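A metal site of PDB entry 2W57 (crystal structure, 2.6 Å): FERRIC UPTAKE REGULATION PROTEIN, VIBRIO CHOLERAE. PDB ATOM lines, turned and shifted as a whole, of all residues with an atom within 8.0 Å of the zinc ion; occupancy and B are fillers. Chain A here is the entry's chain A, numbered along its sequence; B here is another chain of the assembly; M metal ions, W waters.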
ATOM      1  N   HIS A  87      14.414   3.344  -3.842  1.00  0.00           N
ATOM      2  CA  HIS A  87      14.461   2.096  -3.098  1.00  0.00           C
ATOM      3  C   HIS A  87      15.465   2.135  -1.961  1.00  0.00           C
ATOM      4  O   HIS A  87      16.606   2.568  -2.148  1.00  0.00           O
ATOM      5  CB  HIS A  87      14.816   0.953  -4.052  1.00  0.00           C
ATOM      6  CG  HIS A  87      15.039  -0.355  -3.362  1.00  0.00           C
ATOM      7  ND1 HIS A  87      13.996  -1.224  -3.067  1.00  0.00           N
ATOM      8  CD2 HIS A  87      16.169  -0.948  -2.920  1.00  0.00           C
ATOM      9  CE1 HIS A  87      14.485  -2.295  -2.460  1.00  0.00           C
ATOM     10  NE2 HIS A  87      15.804  -2.148  -2.357  1.00  0.00           N
ATOM     11  N   HIS A  88      15.046   1.680  -0.777  1.00  0.00           N
ATOM     12  CA  HIS A  88      15.984   1.372   0.293  1.00  0.00           C
ATOM     13  C   HIS A  88      15.570   0.135   1.122  1.00  0.00           C
ATOM     14  O   HIS A  88      14.459  -0.402   0.996  1.00  0.00           O
ATOM     15  CB  HIS A  88      16.245   2.610   1.178  1.00  0.00           C
ATOM     16  CG  HIS A  88      15.019   3.166   1.831  1.00  0.00           C
ATOM     17  ND1 HIS A  88      14.079   3.907   1.151  1.00  0.00           N
ATOM     18  CD2 HIS A  88      14.588   3.107   3.113  1.00  0.00           C
ATOM     19  CE1 HIS A  88      13.118   4.276   1.980  1.00  0.00           C
ATOM     20  NE2 HIS A  88      13.400   3.802   3.181  1.00  0.00           N
ATOM     21  N   ASP A  89      16.513  -0.353   1.928  1.00  0.00           N
ATOM     22  CA  ASP A  89      16.263  -1.415   2.885  1.00  0.00           C
ATOM     23  C   ASP A  89      16.522  -0.856   4.266  1.00  0.00           C
ATOM     24  O   ASP A  89      16.888   0.318   4.389  1.00  0.00           O
ATOM     25  CB  ASP A  89      17.143  -2.616   2.570  1.00  0.00           C
ATOM     26  CG  ASP A  89      16.843  -3.172   1.220  1.00  0.00           C
ATOM     27  OD1 ASP A  89      15.656  -3.459   0.961  1.00  0.00           O
ATOM     28  OD2 ASP A  89      17.773  -3.297   0.399  1.00  0.00           O
ATOM     29  N   HIS A  90      16.327  -1.663   5.299  1.00  0.00           N
ATOM     30  CA  HIS A  90      16.272  -1.112   6.640  1.00  0.00           C
ATOM     31  C   HIS A  90      17.122  -1.855   7.637  1.00  0.00           C
ATOM     32  O   HIS A  90      17.121  -3.082   7.690  1.00  0.00           O
ATOM     33  CB  HIS A  90      14.835  -1.010   7.141  1.00  0.00           C
ATOM     34  CG  HIS A  90      13.897  -0.354   6.173  1.00  0.00           C
ATOM     35  ND1 HIS A  90      13.360  -1.030   5.090  1.00  0.00           N
ATOM     36  CD2 HIS A  90      13.406   0.906   6.107  1.00  0.00           C
ATOM     37  CE1 HIS A  90      12.578  -0.206   4.405  1.00  0.00           C
ATOM     38  NE2 HIS A  90      12.586   0.973   5.003  1.00  0.00           N
ATOM     39  N   PHE A 102      19.535   1.851   3.921  1.00  0.00           N
ATOM     40  CA  PHE A 102      20.715   1.555   3.102  1.00  0.00           C
ATOM     41  C   PHE A 102      20.295   0.945   1.775  1.00  0.00           C
ATOM     42  O   PHE A 102      19.179   0.453   1.625  1.00  0.00           O
ATOM     43  CB  PHE A 102      21.698   0.640   3.859  1.00  0.00           C
ATOM     44  CG  PHE A 102      21.205  -0.778   4.043  1.00  0.00           C
ATOM     45  CD1 PHE A 102      20.396  -1.108   5.138  1.00  0.00           C
ATOM     46  CD2 PHE A 102      21.559  -1.773   3.140  1.00  0.00           C
ATOM     47  CE1 PHE A 102      19.943  -2.412   5.322  1.00  0.00           C
ATOM     48  CE2 PHE A 102      21.096  -3.085   3.317  1.00  0.00           C
ATOM     49  CZ  PHE A 102      20.294  -3.396   4.412  1.00  0.00           C
ATOM     50  N   SER A 103      21.214   0.972   0.812  1.00  0.00           N
ATOM     51  CA  SER A 103      21.008   0.342  -0.474  1.00  0.00           C
ATOM     52  C   SER A 103      22.347  -0.170  -1.022  1.00  0.00           C
ATOM     53  O   SER A 103      23.061   0.551  -1.708  1.00  0.00           O
ATOM     54  CB  SER A 103      20.341   1.318  -1.456  1.00  0.00           C
ATOM     55  OG  SER A 103      20.009   0.657  -2.671  1.00  0.00           O
ATOM     56  N   ASP A 104      22.665  -1.413  -0.700  1.00  0.00           N
ATOM     57  CA  ASP A 104      23.918  -2.023  -1.084  1.00  0.00           C
ATOM     58  C   ASP A 104      23.829  -2.640  -2.477  1.00  0.00           C
ATOM     59  O   ASP A 104      22.898  -3.397  -2.764  1.00  0.00           O
ATOM     60  CB  ASP A 104      24.272  -3.103  -0.065  1.00  0.00           C
ATOM     61  CG  ASP A 104      25.683  -3.620  -0.212  1.00  0.00           C
ATOM     62  OD1 ASP A 104      26.634  -2.828   0.020  1.00  0.00           O
ATOM     63  OD2 ASP A 104      25.849  -4.807  -0.560  1.00  0.00           O
ATOM     64  N   ILE A 107      24.481  -6.726  -2.456  1.00  0.00           N
ATOM     65  CA  ILE A 107      23.240  -7.379  -2.038  1.00  0.00           C
ATOM     66  C   ILE A 107      22.195  -7.288  -3.149  1.00  0.00           C
ATOM     67  O   ILE A 107      21.629  -8.318  -3.545  1.00  0.00           O
ATOM     68  CB  ILE A 107      22.693  -6.818  -0.715  1.00  0.00           C
ATOM     69  CG1 ILE A 107      23.648  -7.153   0.436  1.00  0.00           C
ATOM     70  CG2 ILE A 107      21.276  -7.356  -0.430  1.00  0.00           C
ATOM     71  CD1 ILE A 107      23.369  -6.409   1.700  1.00  0.00           C
ATOM     72  N   GLU A 108      21.950  -6.090  -3.674  1.00  0.00           N
ATOM     73  CA  GLU A 108      20.984  -5.952  -4.755  1.00  0.00           C
ATOM     74  C   GLU A 108      21.276  -6.934  -5.887  1.00  0.00           C
ATOM     75  O   GLU A 108      20.371  -7.635  -6.330  1.00  0.00           O
ATOM     76  CB  GLU A 108      20.909  -4.505  -5.289  1.00  0.00           C
ATOM     77  CG  GLU A 108      20.315  -3.460  -4.326  1.00  0.00           C
ATOM     78  CD  GLU A 108      19.024  -3.907  -3.629  1.00  0.00           C
ATOM     79  OE1 GLU A 108      18.189  -4.599  -4.235  1.00  0.00           O
ATOM     80  OE2 GLU A 108      18.856  -3.549  -2.444  1.00  0.00           O
ATOM     81  N   GLN A 111      20.705 -10.921  -4.953  1.00  0.00           N
ATOM     82  CA  GLN A 111      19.271 -11.262  -4.984  1.00  0.00           C
ATOM     83  C   GLN A 111      18.811 -11.709  -6.380  1.00  0.00           C
ATOM     84  O   GLN A 111      18.121 -12.729  -6.506  1.00  0.00           O
ATOM     85  CB  GLN A 111      18.437 -10.068  -4.477  1.00  0.00           C
ATOM     86  CG  GLN A 111      18.743  -9.652  -3.028  1.00  0.00           C
ATOM     87  CD  GLN A 111      17.959  -8.433  -2.551  1.00  0.00           C
ATOM     88  OE1 GLN A 111      17.325  -7.744  -3.341  1.00  0.00           O
ATOM     89  NE2 GLN A 111      18.030  -8.147  -1.255  1.00  0.00           N
ATOM     90  N   ASN A 124      10.050  -8.147  -6.631  1.00  0.00           N
ATOM     91  CA  ASN A 124      10.177  -7.288  -5.457  1.00  0.00           C
ATOM     92  C   ASN A 124      10.891  -8.058  -4.355  1.00  0.00           C
ATOM     93  O   ASN A 124      10.987  -9.286  -4.411  1.00  0.00           O
ATOM     94  CB  ASN A 124       8.786  -6.831  -4.999  1.00  0.00           C
ATOM     95  CG  ASN A 124       8.834  -5.711  -3.965  1.00  0.00           C
ATOM     96  OD1 ASN A 124       9.886  -5.124  -3.720  1.00  0.00           O
ATOM     97  ND2 ASN A 124       7.686  -5.425  -3.349  1.00  0.00           N
ATOM     98  N   HIS A 125      11.412  -7.334  -3.361  1.00  0.00           N
ATOM     99  CA  HIS A 125      12.009  -7.948  -2.172  1.00  0.00           C
ATOM    100  C   HIS A 125      11.797  -7.068  -0.948  1.00  0.00           C
ATOM    101  O   HIS A 125      11.363  -5.923  -1.060  1.00  0.00           O
ATOM    102  CB  HIS A 125      13.495  -8.237  -2.404  1.00  0.00           C
ATOM    103  CG  HIS A 125      14.361  -7.013  -2.441  1.00  0.00           C
ATOM    104  ND1 HIS A 125      14.534  -6.272  -3.588  1.00  0.00           N
ATOM    105  CD2 HIS A 125      15.120  -6.423  -1.491  1.00  0.00           C
ATOM    106  CE1 HIS A 125      15.353  -5.266  -3.345  1.00  0.00           C
ATOM    107  NE2 HIS A 125      15.733  -5.341  -2.075  1.00  0.00           N
ATOM    108  N   SER A 126      12.077  -7.594   0.240  1.00  0.00           N
ATOM    109  CA  SER A 126      12.167  -6.754   1.425  1.00  0.00           C
ATOM    110  C   SER A 126      13.241  -7.299   2.336  1.00  0.00           C
ATOM    111  O   SER A 126      13.340  -8.508   2.522  1.00  0.00           O
ATOM    112  CB  SER A 126      10.818  -6.631   2.158  1.00  0.00           C
ATOM    113  OG  SER A 126      10.337  -7.896   2.587  1.00  0.00           O
ATOM    114  N   LEU A 127      14.050  -6.396   2.888  1.00  0.00           N
ATOM    115  CA  LEU A 127      15.184  -6.792   3.743  1.00  0.00           C
ATOM    116  C   LEU A 127      15.238  -5.940   4.995  1.00  0.00           C
ATOM    117  O   LEU A 127      15.272  -4.713   4.917  1.00  0.00           O
ATOM    118  CB  LEU A 127      16.514  -6.728   2.959  1.00  0.00           C
ATOM    119  CG  LEU A 127      17.860  -6.783   3.671  1.00  0.00           C
ATOM    120  CD1 LEU A 127      18.089  -8.125   4.335  1.00  0.00           C
ATOM    121  CD2 LEU A 127      18.990  -6.480   2.689  1.00  0.00           C
ATOM    122  N   LEU B 127      14.938 -11.750   5.075  1.00  0.00           N
ATOM    123  CA  LEU B 127      15.123 -11.456   3.654  1.00  0.00           C
ATOM    124  C   LEU B 127      14.098 -12.220   2.827  1.00  0.00           C
ATOM    125  O   LEU B 127      14.186 -13.444   2.677  1.00  0.00           O
ATOM    126  CB  LEU B 127      16.548 -11.787   3.217  1.00  0.00           C
ATOM    127  CG  LEU B 127      16.987 -11.824   1.740  1.00  0.00           C
ATOM    128  CD1 LEU B 127      16.663 -10.523   1.009  1.00  0.00           C
ATOM    129  CD2 LEU B 127      18.484 -12.139   1.646  1.00  0.00           C
ATOM    130  N   LEU B 129      12.501 -12.516  -0.834  1.00  0.00           N
ATOM    131  CA  LEU B 129      12.563 -12.222  -2.242  1.00  0.00           C
ATOM    132  C   LEU B 129      11.240 -12.704  -2.832  1.00  0.00           C
ATOM    133  O   LEU B 129      10.837 -13.846  -2.604  1.00  0.00           O
ATOM    134  CB  LEU B 129      13.754 -12.947  -2.901  1.00  0.00           C
ATOM    135  CG  LEU B 129      15.182 -12.659  -2.412  1.00  0.00           C
ATOM    136  CD1 LEU B 129      16.237 -13.452  -3.192  1.00  0.00           C
ATOM    137  CD2 LEU B 129      15.512 -11.165  -2.434  1.00  0.00           C
HETATM  138 ZN    ZN M   1      17.077  -3.745  -1.368  1.00  0.00          ZN
HETATM  139  O   HOH W   1      20.374  -3.693  -0.252  1.00  0.00           O
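The backbone carbonyl oxygen (O) of Phe 102 lies within hydrogen-bond range of the backbone NH (N) of Asp 89, at 2.8 Å. OE1 of Gln 111 sits close to OE1 of Glu 108, 3.4 Å away. ND1 of His 125 sits at hydrogen-bond distance from OE1 of Gln 111, at 3.2 Å.
Of the 16 residues printed, 4 come within 4 Å of the zinc ion.
The zinc ion is bound by OD2 of Asp 89, OE2 of Glu 108, NE2 of His 125 and NE2 of His 87. Slightly farther from the zinc ion lies the side-chain carboxylate (OD1) of Asp 89 (2.7 Å).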
